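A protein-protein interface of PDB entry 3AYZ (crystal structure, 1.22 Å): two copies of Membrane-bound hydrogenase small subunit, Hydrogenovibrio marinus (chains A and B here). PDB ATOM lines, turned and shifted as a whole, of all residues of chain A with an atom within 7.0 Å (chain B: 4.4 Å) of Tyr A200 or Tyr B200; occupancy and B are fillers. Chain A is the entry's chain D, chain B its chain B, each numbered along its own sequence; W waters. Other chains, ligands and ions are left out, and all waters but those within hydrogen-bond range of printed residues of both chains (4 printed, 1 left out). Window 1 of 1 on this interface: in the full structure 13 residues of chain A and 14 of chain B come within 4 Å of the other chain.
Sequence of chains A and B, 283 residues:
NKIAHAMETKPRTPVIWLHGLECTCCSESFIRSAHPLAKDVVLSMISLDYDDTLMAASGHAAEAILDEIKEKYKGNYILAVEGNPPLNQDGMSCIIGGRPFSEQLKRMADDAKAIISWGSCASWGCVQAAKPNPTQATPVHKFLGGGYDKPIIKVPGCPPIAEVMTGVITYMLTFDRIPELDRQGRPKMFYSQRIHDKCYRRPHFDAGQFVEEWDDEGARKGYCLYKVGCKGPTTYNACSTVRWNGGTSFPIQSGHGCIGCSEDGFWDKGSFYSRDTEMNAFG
Among the printed residues, pairs that only touch across the chains: His A196 with Pro B203 (3.3 Å), Asp A197 with Pro B203 (3.2 Å), Lys A198 with Tyr B200 (3.2 Å), Lys A198 with Arg B201 (3.9 Å), Lys A198 with Pro B203 (3.8 Å), Cys A199 with Tyr B200 (3.9 Å), Cys A199 with Pro B203 (3.98 Å), Tyr A200 with Lys B198 (3.2 Å), Tyr A200 with Cys B199 (3.9 Å), Tyr A200 with Tyr B200 (3.8 Å), Arg A202 with Pro B203 (3.4 Å), Pro A203 with Asp B197 (3.2 Å), Pro A203 with Lys B198 (3.7 Å), Pro A203 with Cys B199 (3.98 Å), Pro A203 with Arg B202 (3.4 Å), His A204 with Asp B197 (3.9 Å) and Gly A222 with Lys B198 (3.7 Å).
The side-chain amino group (NZ) of Lys B198 lies within hydrogen-bond range of a ring nitrogen (NE2) of His A204, at 2.7 Å.
Lys A198 touches Tyr B200, and with the chains exchanged Tyr A200 touches Lys B198.
Cys A199 touches Tyr B200, and with the chains exchanged Tyr A200 touches Cys B199.
Cys A199 touches Pro B203, and with the chains exchanged Pro A203 touches Cys B199.
Arg A202 touches Pro B203, and with the chains exchanged Pro A203 touches Arg B202.
Positions printed for both chains: 197, 198, 199, 200, 201, 202, 203, 250, 252 and 253.
Hydrophobic or aromatic side chains of chain B that line the printed part of chain A: Tyr B200 and Pro B203.
Printed residues of chain A that touch a printed residue of chain B: His A196, Asp A197, Lys A198, Cys A199, Tyr A200, Arg A202, Pro A203, His A204 and Gly A222.
Along chain A the printed residues that touch a printed residue of chain B span positions 196 to 222.
Among the printed residues, 18 pairs touch across the chains.
Water W2 bridges OE1 of Gln B253 (2.7 Å) and NH2 of Arg A243 (3.1 Å).
Water W1 bridges the backbone carbonyl oxygen (O) of Pro A203 (2.8 Å) and the guanidinium group (NH2) of Arg B202 (2.9 Å).
Water W3 lies within hydrogen-bond range of the backbone carbonyl oxygen of Pro B203 (2.8 Å) and the guanidinium group of Arg A202 (2.9 Å).
Water W4 lies within hydrogen-bond range of O of Thr A241 (2.9 Å), NE2 of Gln B253 (3.0 Å) and NH1 of Arg A243 (3.4 Å).
Of the printed residues of chain B, Tyr A200 touches Lys B198 (3.2 Å), Cys B199 (3.9 Å) and Tyr B200 (3.8 Å).
Arg A201 touches none of the printed residues of chain B.
Of the printed residues of chain B, His A204 touches Asp B197 (3.9 Å) and Lys B198 (2.7 Å).
Tyr A223 touches none of the printed residues of chain B.
Printed residues of chain A within 4 Å of Lys B198: Tyr A200, Pro A203, His A204 and Gly A222.
Printed residues of chain A within 4 Å of Tyr B200: Lys A198, Cys A199 and Tyr A200.
The nearest printed residue of chain A that does not touch Tyr B200 is Asp A197 (4.3 Å).
The side-chain sulfur (SG) of Cys B199 lies close to the backbone NH (N) of Arg B201 (3.5 Å).
The backbone carbonyl oxygen of His A196 lies within hydrogen-bond range of the guanidinium group of Arg A202, at 3.2 Å.
NH1 of Arg B201 lies within hydrogen-bond range of O of Ile B252.
The side-chain hydroxyl (OG) of Ser A240 sits close to the backbone carbonyl oxygen (O) of Lys A198.
The side-chain hydroxyl of Tyr B200 lies within hydrogen-bond range of the guanidinium group of Arg B201 (2.9 Å).
SG of Cys A199 lies close to N of Arg A201.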
ATOM      1  N   ILE A 195      10.221  -0.840  27.346  1.00  0.00           N
ATOM      2  CA  ILE A 195      10.044   0.614  27.512  1.00  0.00           C
ATOM      3  C   ILE A 195       8.616   1.004  27.245  1.00  0.00           C
ATOM      4  O   ILE A 195       7.979   1.735  28.026  1.00  0.00           O
ATOM      5  CB  ILE A 195      11.008   1.395  26.606  1.00  0.00           C
ATOM      6  CG1 ILE A 195      12.485   1.089  26.716  1.00  0.00           C
ATOM      7  CG2 ILE A 195      10.791   2.910  26.801  1.00  0.00           C
ATOM      8  CD1 ILE A 195      13.017   1.204  28.127  1.00  0.00           C
ATOM      9  N   HIS A 196       8.048   0.504  26.145  1.00  0.00           N
ATOM     10  CA  HIS A 196       6.720   0.763  25.613  1.00  0.00           C
ATOM     11  C   HIS A 196       5.606   0.265  26.543  1.00  0.00           C
ATOM     12  O   HIS A 196       4.468   0.757  26.450  1.00  0.00           O
ATOM     13  CB  HIS A 196       6.591   0.190  24.232  1.00  0.00           C
ATOM     14  CG  HIS A 196       5.359   0.407  23.431  1.00  0.00           C
ATOM     15  ND1 HIS A 196       5.044   1.622  22.782  1.00  0.00           N
ATOM     16  CD2 HIS A 196       4.407  -0.480  23.083  1.00  0.00           C
ATOM     17  CE1 HIS A 196       3.887   1.417  22.087  1.00  0.00           C
ATOM     18  NE2 HIS A 196       3.514   0.177  22.267  1.00  0.00           N
ATOM     19  N   ASP A 197       5.942  -0.719  27.386  1.00  0.00           N
ATOM     20  CA  ASP A 197       4.999  -1.283  28.331  1.00  0.00           C
ATOM     21  C   ASP A 197       4.801  -0.409  29.579  1.00  0.00           C
ATOM     22  O   ASP A 197       3.916  -0.707  30.376  1.00  0.00           O
ATOM     23  CB  ASP A 197       5.503  -2.645  28.802  1.00  0.00           C
ATOM     24  CG  ASP A 197       5.707  -3.726  27.837  1.00  0.00           C
ATOM     25  OD1 ASP A 197       4.966  -3.752  26.816  1.00  0.00           O
ATOM     26  OD2 ASP A 197       6.546  -4.685  28.129  1.00  0.00           O
ATOM     27  N   LYS A 198       5.593   0.651  29.715  1.00  0.00           N
ATOM     28  CA  LYS A 198       5.469   1.596  30.858  1.00  0.00           C
ATOM     29  C   LYS A 198       5.825   3.007  30.364  1.00  0.00           C
ATOM     30  O   LYS A 198       6.323   3.821  31.130  1.00  0.00           O
ATOM     31  CB  LYS A 198       6.225   1.173  32.089  1.00  0.00           C
ATOM     32  CG  LYS A 198       5.689   0.086  33.056  1.00  0.00           C
ATOM     33  CD  LYS A 198       4.371   0.417  33.755  1.00  0.00           C
ATOM     34  CE  LYS A 198       4.251  -0.384  35.087  1.00  0.00           C
ATOM     35  NZ  LYS A 198       3.945   0.269  36.421  1.00  0.00           N
ATOM     36  N   CYS A 199       5.517   3.351  29.133  1.00  0.00           N
ATOM     37  CA  CYS A 199       5.882   4.633  28.557  1.00  0.00           C
ATOM     38  C   CYS A 199       4.770   5.670  28.757  1.00  0.00           C
ATOM     39  O   CYS A 199       3.641   5.465  28.228  1.00  0.00           O
ATOM     40  CB  CYS A 199       6.224   4.514  27.070  1.00  0.00           C
ATOM     41  SG  CYS A 199       6.813   6.082  26.391  1.00  0.00           S
ATOM     42  N   TYR A 200       5.078   6.795  29.350  1.00  0.00           N
ATOM     43  CA  TYR A 200       4.120   7.880  29.569  1.00  0.00           C
ATOM     44  C   TYR A 200       3.617   8.529  28.262  1.00  0.00           C
ATOM     45  O   TYR A 200       2.616   9.204  28.330  1.00  0.00           O
ATOM     46  CB  TYR A 200       4.725   8.916  30.541  1.00  0.00           C
ATOM     47  CG  TYR A 200       5.599   9.915  29.809  1.00  0.00           C
ATOM     48  CD1 TYR A 200       5.186  11.235  29.577  1.00  0.00           C
ATOM     49  CD2 TYR A 200       6.843   9.568  29.291  1.00  0.00           C
ATOM     50  CE1 TYR A 200       5.963  12.162  28.925  1.00  0.00           C
ATOM     51  CE2 TYR A 200       7.579  10.459  28.602  1.00  0.00           C
ATOM     52  CZ  TYR A 200       7.155  11.762  28.391  1.00  0.00           C
ATOM     53  OH  TYR A 200       7.934  12.623  27.663  1.00  0.00           O
ATOM     54  N   ARG A 201       4.274   8.310  27.126  1.00  0.00           N
ATOM     55  CA  ARG A 201       3.759   8.795  25.838  1.00  0.00           C
ATOM     56  C   ARG A 201       2.783   7.831  25.184  1.00  0.00           C
ATOM     57  O   ARG A 201       2.220   8.076  24.113  1.00  0.00           O
ATOM     58  CB  ARG A 201       4.891   9.199  24.868  1.00  0.00           C
ATOM     59  CG  ARG A 201       5.750  10.313  25.392  1.00  0.00           C
ATOM     60  CD  ARG A 201       6.640  10.901  24.286  1.00  0.00           C
ATOM     61  NE  ARG A 201       7.498  11.971  24.790  1.00  0.00           N
ATOM     62  CZ  ARG A 201       8.012  12.941  24.024  1.00  0.00           C
ATOM     63  NH1 ARG A 201       7.805  13.033  22.745  1.00  0.00           N
ATOM     64  NH2 ARG A 201       8.789  13.857  24.608  1.00  0.00           N
ATOM     65  N   ARG A 202       2.586   6.637  25.820  1.00  0.00           N
ATOM     66  CA  ARG A 202       1.690   5.639  25.260  1.00  0.00           C
ATOM     67  C   ARG A 202       0.290   6.223  24.952  1.00  0.00           C
ATOM     68  O   ARG A 202      -0.284   5.795  23.907  1.00  0.00           O
ATOM     69  CB  ARG A 202       1.572   4.431  26.178  1.00  0.00           C
ATOM     70  CG  ARG A 202       0.672   3.323  25.646  1.00  0.00           C
ATOM     71  CD  ARG A 202       1.254   2.657  24.375  1.00  0.00           C
ATOM     72  NE  ARG A 202       0.366   1.515  24.104  1.00  0.00           N
ATOM     73  CZ  ARG A 202       0.612   0.249  24.519  1.00  0.00           C
ATOM     74  NH1 ARG A 202      -0.289  -0.663  24.280  1.00  0.00           N
ATOM     75  NH2 ARG A 202       1.724  -0.106  25.153  1.00  0.00           N
ATOM     76  N   PRO A 203      -0.310   7.087  25.761  1.00  0.00           N
ATOM     77  CA  PRO A 203      -1.623   7.616  25.364  1.00  0.00           C
ATOM     78  C   PRO A 203      -1.645   8.219  23.953  1.00  0.00           C
ATOM     79  O   PRO A 203      -2.632   8.089  23.214  1.00  0.00           O
ATOM     80  CB  PRO A 203      -1.913   8.661  26.410  1.00  0.00           C
ATOM     81  CG  PRO A 203      -1.176   8.147  27.644  1.00  0.00           C
ATOM     82  CD  PRO A 203       0.101   7.580  27.101  1.00  0.00           C
ATOM     83  N   HIS A 204      -0.542   8.819  23.548  1.00  0.00           N
ATOM     84  CA  HIS A 204      -0.421   9.409  22.228  1.00  0.00           C
ATOM     85  C   HIS A 204      -0.283   8.358  21.160  1.00  0.00           C
ATOM     86  O   HIS A 204      -0.963   8.389  20.128  1.00  0.00           O
ATOM     87  CB  HIS A 204       0.749  10.428  22.197  1.00  0.00           C
ATOM     88  CG  HIS A 204       0.532  11.582  23.069  1.00  0.00           C
ATOM     89  ND1 HIS A 204      -0.555  12.402  22.991  1.00  0.00           N
ATOM     90  CD2 HIS A 204       1.286  12.091  24.077  1.00  0.00           C
ATOM     91  CE1 HIS A 204      -0.461  13.328  23.912  1.00  0.00           C
ATOM     92  NE2 HIS A 204       0.653  13.190  24.610  1.00  0.00           N
ATOM     93  N   GLY A 222       4.850  16.601  23.155  1.00  0.00           N
ATOM     94  CA  GLY A 222       5.308  15.307  23.677  1.00  0.00           C
ATOM     95  C   GLY A 222       4.606  14.095  23.087  1.00  0.00           C
ATOM     96  O   GLY A 222       4.419  13.092  23.807  1.00  0.00           O
ATOM     97  N   TYR A 223       4.236  14.112  21.823  1.00  0.00           N
ATOM     98  CA  TYR A 223       3.598  13.023  21.148  1.00  0.00           C
ATOM     99  C   TYR A 223       4.572  11.832  21.003  1.00  0.00           C
ATOM    100  O   TYR A 223       5.766  11.902  21.153  1.00  0.00           O
ATOM    101  CB  TYR A 223       3.055  13.431  19.777  1.00  0.00           C
ATOM    102  CG  TYR A 223       1.780  14.214  19.773  1.00  0.00           C
ATOM    103  CD1 TYR A 223       1.132  14.640  20.940  1.00  0.00           C
ATOM    104  CD2 TYR A 223       1.168  14.519  18.573  1.00  0.00           C
ATOM    105  CE1 TYR A 223      -0.036  15.358  20.909  1.00  0.00           C
ATOM    106  CE2 TYR A 223      -0.011  15.217  18.544  1.00  0.00           C
ATOM    107  CZ  TYR A 223      -0.661  15.650  19.692  1.00  0.00           C
ATOM    108  OH  TYR A 223      -1.831  16.343  19.648  1.00  0.00           O
ATOM    109  N   SER A 240      11.802   3.763  31.420  1.00  0.00           N
ATOM    110  CA  SER A 240      10.508   4.417  31.572  1.00  0.00           C
ATOM    111  C   SER A 240       9.902   4.311  32.942  1.00  0.00           C
ATOM    112  O   SER A 240       8.844   4.893  33.193  1.00  0.00           O
ATOM    113  CB  SER A 240       9.575   3.935  30.458  1.00  0.00           C
ATOM    114  OG  SER A 240       9.452   2.514  30.475  1.00  0.00           O
ATOM    115  N   THR A 241      10.613   3.622  33.859  1.00  0.00           N
ATOM    116  CA  THR A 241      10.144   3.411  35.224  1.00  0.00           C
ATOM    117  C   THR A 241      11.099   4.021  36.218  1.00  0.00           C
ATOM    118  O   THR A 241      10.690   4.934  36.998  1.00  0.00           O
ATOM    119  CB  THR A 241       9.907   1.883  35.500  1.00  0.00           C
ATOM    120  OG1 THR A 241      11.062   1.156  35.009  1.00  0.00           O
ATOM    121  CG2 THR A 241       8.622   1.402  34.817  1.00  0.00           C
ATOM    122  N   ARG A 243      14.068   5.444  35.177  1.00  0.00           N
ATOM    123  CA  ARG A 243      14.575   6.594  34.492  1.00  0.00           C
ATOM    124  C   ARG A 243      16.040   6.850  34.861  1.00  0.00           C
ATOM    125  O   ARG A 243      16.689   5.991  35.516  1.00  0.00           O
ATOM    126  CB  ARG A 243      13.687   7.859  34.676  1.00  0.00           C
ATOM    127  CG  ARG A 243      12.226   7.579  34.349  1.00  0.00           C
ATOM    128  CD  ARG A 243      11.342   8.906  34.394  1.00  0.00           C
ATOM    129  NE  ARG A 243      11.552   9.571  35.651  1.00  0.00           N
ATOM    130  CZ  ARG A 243      11.167   9.156  36.868  1.00  0.00           C
ATOM    131  NH1 ARG A 243      10.405   8.107  37.029  1.00  0.00           N
ATOM    132  NH2 ARG A 243      11.584   9.836  37.916  1.00  0.00           N
ATOM    133  N   PHE A 250      14.616  10.394  30.561  1.00  0.00           N
ATOM    134  CA  PHE A 250      15.077   9.232  29.801  1.00  0.00           C
ATOM    135  C   PHE A 250      15.004   9.686  28.330  1.00  0.00           C
ATOM    136  O   PHE A 250      14.441  10.759  28.015  1.00  0.00           O
ATOM    137  CB  PHE A 250      14.303   7.970  30.080  1.00  0.00           C
ATOM    138  CG  PHE A 250      12.872   7.824  29.678  1.00  0.00           C
ATOM    139  CD1 PHE A 250      12.463   6.865  28.777  1.00  0.00           C
ATOM    140  CD2 PHE A 250      11.873   8.635  30.268  1.00  0.00           C
ATOM    141  CE1 PHE A 250      11.166   6.632  28.431  1.00  0.00           C
ATOM    142  CE2 PHE A 250      10.544   8.414  29.933  1.00  0.00           C
ATOM    143  CZ  PHE A 250      10.195   7.436  29.038  1.00  0.00           C
ATOM    144  N   ILE A 252      13.231   9.173  25.646  1.00  0.00           N
ATOM    145  CA  ILE A 252      11.909   9.535  25.126  1.00  0.00           C
ATOM    146  C   ILE A 252      11.408  10.788  25.758  1.00  0.00           C
ATOM    147  O   ILE A 252      10.865  11.669  25.055  1.00  0.00           O
ATOM    148  CB  ILE A 252      10.963   8.336  25.291  1.00  0.00           C
ATOM    149  CG1 ILE A 252      11.304   7.200  24.287  1.00  0.00           C
ATOM    150  CG2 ILE A 252       9.501   8.780  25.199  1.00  0.00           C
ATOM    151  CD1 ILE A 252      11.058   5.867  24.776  1.00  0.00           C
ATOM    152  N   GLN A 253      11.581  10.980  27.070  1.00  0.00           N
ATOM    153  CA  GLN A 253      11.112  12.210  27.690  1.00  0.00           C
ATOM    154  C   GLN A 253      11.742  13.428  27.052  1.00  0.00           C
ATOM    155  O   GLN A 253      11.115  14.437  26.800  1.00  0.00           O
ATOM    156  CB  GLN A 253      11.388  12.195  29.209  1.00  0.00           C
ATOM    157  CG  GLN A 253      10.934  13.505  29.854  1.00  0.00           C
ATOM    158  CD  GLN A 253      11.050  13.516  31.366  1.00  0.00           C
ATOM    159  OE1 GLN A 253      11.243  12.481  32.008  1.00  0.00           O
ATOM    160  NE2 GLN A 253      10.833  14.654  31.942  1.00  0.00           N
ATOM    161  N   SER A 254      13.042  13.336  26.755  1.00  0.00           N
ATOM    162  CA  SER A 254      13.794  14.407  26.148  1.00  0.00           C
ATOM    163  C   SER A 254      13.639  14.492  24.665  1.00  0.00           C
ATOM    164  O   SER A 254      14.216  15.393  24.040  1.00  0.00           O
ATOM    165  CB  SER A 254      15.272  14.301  26.567  1.00  0.00           C
ATOM    166  OG  SER A 254      15.450  14.426  27.977  1.00  0.00           O
ATOM    167  N   GLY A 255      12.827  13.660  24.027  1.00  0.00           N
ATOM    168  CA  GLY A 255      12.426  13.859  22.644  1.00  0.00           C
ATOM    169  C   GLY A 255      13.029  12.999  21.573  1.00  0.00           C
ATOM    170  O   GLY A 255      12.711  13.211  20.419  1.00  0.00           O
ATOM    171  N   ASP B 197      -3.696  11.076  30.031  1.00  0.00           N
ATOM    172  CA  ASP B 197      -3.146  11.411  28.724  1.00  0.00           C
ATOM    173  C   ASP B 197      -1.616  11.329  28.711  1.00  0.00           C
ATOM    174  O   ASP B 197      -1.029  11.483  27.649  1.00  0.00           O
ATOM    175  CB  ASP B 197      -3.595  12.852  28.358  1.00  0.00           C
ATOM    176  CG  ASP B 197      -4.968  13.299  28.147  1.00  0.00           C
ATOM    177  OD1 ASP B 197      -5.730  12.342  27.727  1.00  0.00           O
ATOM    178  OD2 ASP B 197      -5.364  14.532  28.272  1.00  0.00           O
ATOM    179  N   LYS B 198      -0.976  11.121  29.846  1.00  0.00           N
ATOM    180  CA  LYS B 198       0.494  11.040  29.944  1.00  0.00           C
ATOM    181  C   LYS B 198       0.868  10.051  31.051  1.00  0.00           C
ATOM    182  O   LYS B 198       1.930  10.213  31.707  1.00  0.00           O
ATOM    183  CB  LYS B 198       1.124  12.422  30.114  1.00  0.00           C
ATOM    184  CG  LYS B 198       1.154  13.362  28.908  1.00  0.00           C
ATOM    185  CD  LYS B 198       2.036  12.795  27.825  1.00  0.00           C
ATOM    186  CE  LYS B 198       2.665  13.823  27.025  1.00  0.00           C
ATOM    187  NZ  LYS B 198       1.950  14.897  26.301  1.00  0.00           N
ATOM    188  N   CYS B 199       0.089   9.040  31.308  1.00  0.00           N
ATOM    189  CA  CYS B 199       0.323   8.096  32.397  1.00  0.00           C
ATOM    190  C   CYS B 199       1.136   6.880  31.935  1.00  0.00           C
ATOM    191  O   CYS B 199       0.682   6.192  31.017  1.00  0.00           O
ATOM    192  CB  CYS B 199      -0.958   7.613  33.023  1.00  0.00           C
ATOM    193  SG  CYS B 199      -0.785   6.582  34.457  1.00  0.00           S
ATOM    194  N   TYR B 200       2.212   6.654  32.649  1.00  0.00           N
ATOM    195  CA  TYR B 200       3.094   5.498  32.329  1.00  0.00           C
ATOM    196  C   TYR B 200       2.402   4.142  32.592  1.00  0.00           C
ATOM    197  O   TYR B 200       2.919   3.175  32.062  1.00  0.00           O
ATOM    198  CB  TYR B 200       4.423   5.648  33.127  1.00  0.00           C
ATOM    199  CG  TYR B 200       4.293   5.106  34.531  1.00  0.00           C
ATOM    200  CD1 TYR B 200       4.838   3.900  34.931  1.00  0.00           C
ATOM    201  CD2 TYR B 200       3.543   5.765  35.504  1.00  0.00           C
ATOM    202  CE1 TYR B 200       4.752   3.366  36.190  1.00  0.00           C
ATOM    203  CE2 TYR B 200       3.405   5.231  36.763  1.00  0.00           C
ATOM    204  CZ  TYR B 200       3.974   4.033  37.126  1.00  0.00           C
ATOM    205  OH  TYR B 200       3.740   3.524  38.383  1.00  0.00           O
ATOM    206  N   ARG B 201       1.307   4.070  33.305  1.00  0.00           N
ATOM    207  CA  ARG B 201       0.529   2.845  33.442  1.00  0.00           C
ATOM    208  C   ARG B 201      -0.474   2.592  32.317  1.00  0.00           C
ATOM    209  O   ARG B 201      -1.160   1.580  32.247  1.00  0.00           O
ATOM    210  CB  ARG B 201      -0.157   2.666  34.795  1.00  0.00           C
ATOM    211  CG  ARG B 201       0.847   2.673  35.961  1.00  0.00           C
ATOM    212  CD  ARG B 201       0.162   2.230  37.253  1.00  0.00           C
ATOM    213  NE  ARG B 201       1.100   2.259  38.386  1.00  0.00           N
ATOM    214  CZ  ARG B 201       0.947   1.516  39.492  1.00  0.00           C
ATOM    215  NH1 ARG B 201       1.843   1.661  40.449  1.00  0.00           N
ATOM    216  NH2 ARG B 201      -0.035   0.699  39.675  1.00  0.00           N
ATOM    217  N   ARG B 202      -0.605   3.571  31.411  1.00  0.00           N
ATOM    218  CA  ARG B 202      -1.497   3.438  30.279  1.00  0.00           C
ATOM    219  C   ARG B 202      -1.356   2.168  29.459  1.00  0.00           C
ATOM    220  O   ARG B 202      -2.399   1.602  29.047  1.00  0.00           O
ATOM    221  CB  ARG B 202      -1.415   4.657  29.334  1.00  0.00           C
ATOM    222  CG  ARG B 202      -2.399   4.606  28.201  1.00  0.00           C
ATOM    223  CD  ARG B 202      -3.849   4.771  28.663  1.00  0.00           C
ATOM    224  NE  ARG B 202      -4.665   4.908  27.439  1.00  0.00           N
ATOM    225  CZ  ARG B 202      -5.080   6.024  26.850  1.00  0.00           C
ATOM    226  NH1 ARG B 202      -4.843   7.203  27.427  1.00  0.00           N
ATOM    227  NH2 ARG B 202      -5.725   5.995  25.752  1.00  0.00           N
ATOM    228  N   PRO B 203      -0.145   1.654  29.178  1.00  0.00           N
ATOM    229  CA  PRO B 203      -0.068   0.376  28.458  1.00  0.00           C
ATOM    230  C   PRO B 203      -0.864  -0.717  29.144  1.00  0.00           C
ATOM    231  O   PRO B 203      -1.497  -1.546  28.458  1.00  0.00           O
ATOM    232  CB  PRO B 203       1.405   0.044  28.517  1.00  0.00           C
ATOM    233  CG  PRO B 203       2.082   1.422  28.592  1.00  0.00           C
ATOM    234  CD  PRO B 203       1.184   2.205  29.498  1.00  0.00           C
ATOM    235  N   PHE B 250       4.340  10.165  42.070  1.00  0.00           N
ATOM    236  CA  PHE B 250       3.040  10.800  42.057  1.00  0.00           C
ATOM    237  C   PHE B 250       2.037   9.711  42.571  1.00  0.00           C
ATOM    238  O   PHE B 250       2.451   8.565  42.738  1.00  0.00           O
ATOM    239  CB  PHE B 250       2.655  11.372  40.702  1.00  0.00           C
ATOM    240  CG  PHE B 250       2.343  10.471  39.561  1.00  0.00           C
ATOM    241  CD1 PHE B 250       1.120  10.394  38.938  1.00  0.00           C
ATOM    242  CD2 PHE B 250       3.345   9.658  38.965  1.00  0.00           C
ATOM    243  CE1 PHE B 250       0.830   9.679  37.820  1.00  0.00           C
ATOM    244  CE2 PHE B 250       3.076   8.915  37.842  1.00  0.00           C
ATOM    245  CZ  PHE B 250       1.845   8.890  37.263  1.00  0.00           C
ATOM    246  N   ILE B 252      -0.268   7.717  41.519  1.00  0.00           N
ATOM    247  CA  ILE B 252      -0.402   6.502  40.763  1.00  0.00           C
ATOM    248  C   ILE B 252       0.894   5.690  40.815  1.00  0.00           C
ATOM    249  O   ILE B 252       0.844   4.465  40.970  1.00  0.00           O
ATOM    250  CB  ILE B 252      -0.821   6.825  39.305  1.00  0.00           C
ATOM    251  CG1 ILE B 252      -2.280   7.321  39.259  1.00  0.00           C
ATOM    252  CG2 ILE B 252      -0.504   5.721  38.363  1.00  0.00           C
ATOM    253  CD1 ILE B 252      -2.570   8.366  38.271  1.00  0.00           C
ATOM    254  N   GLN B 253       2.072   6.353  40.735  1.00  0.00           N
ATOM    255  CA  GLN B 253       3.298   5.603  40.824  1.00  0.00           C
ATOM    256  C   GLN B 253       3.360   4.814  42.126  1.00  0.00           C
ATOM    257  O   GLN B 253       3.776   3.648  42.150  1.00  0.00           O
ATOM    258  CB  GLN B 253       4.509   6.490  40.653  1.00  0.00           C
ATOM    259  CG  GLN B 253       5.821   5.723  40.831  1.00  0.00           C
ATOM    260  CD  GLN B 253       7.072   6.533  40.500  1.00  0.00           C
ATOM    261  OE1 GLN B 253       6.987   7.638  39.977  1.00  0.00           O
ATOM    262  NE2 GLN B 253       8.204   5.920  40.737  1.00  0.00           N
HETATM  263  O   HOH W   1      -5.304   8.263  23.927  1.00  0.00           O
HETATM  264  O   HOH W   2       9.096   9.325  39.621  1.00  0.00           O
HETATM  265  O   HOH W   3      -0.532  -2.825  26.132  1.00  0.00           O
HETATM  266  O   HOH W   4      10.957   5.966  39.658  1.00  0.00           O
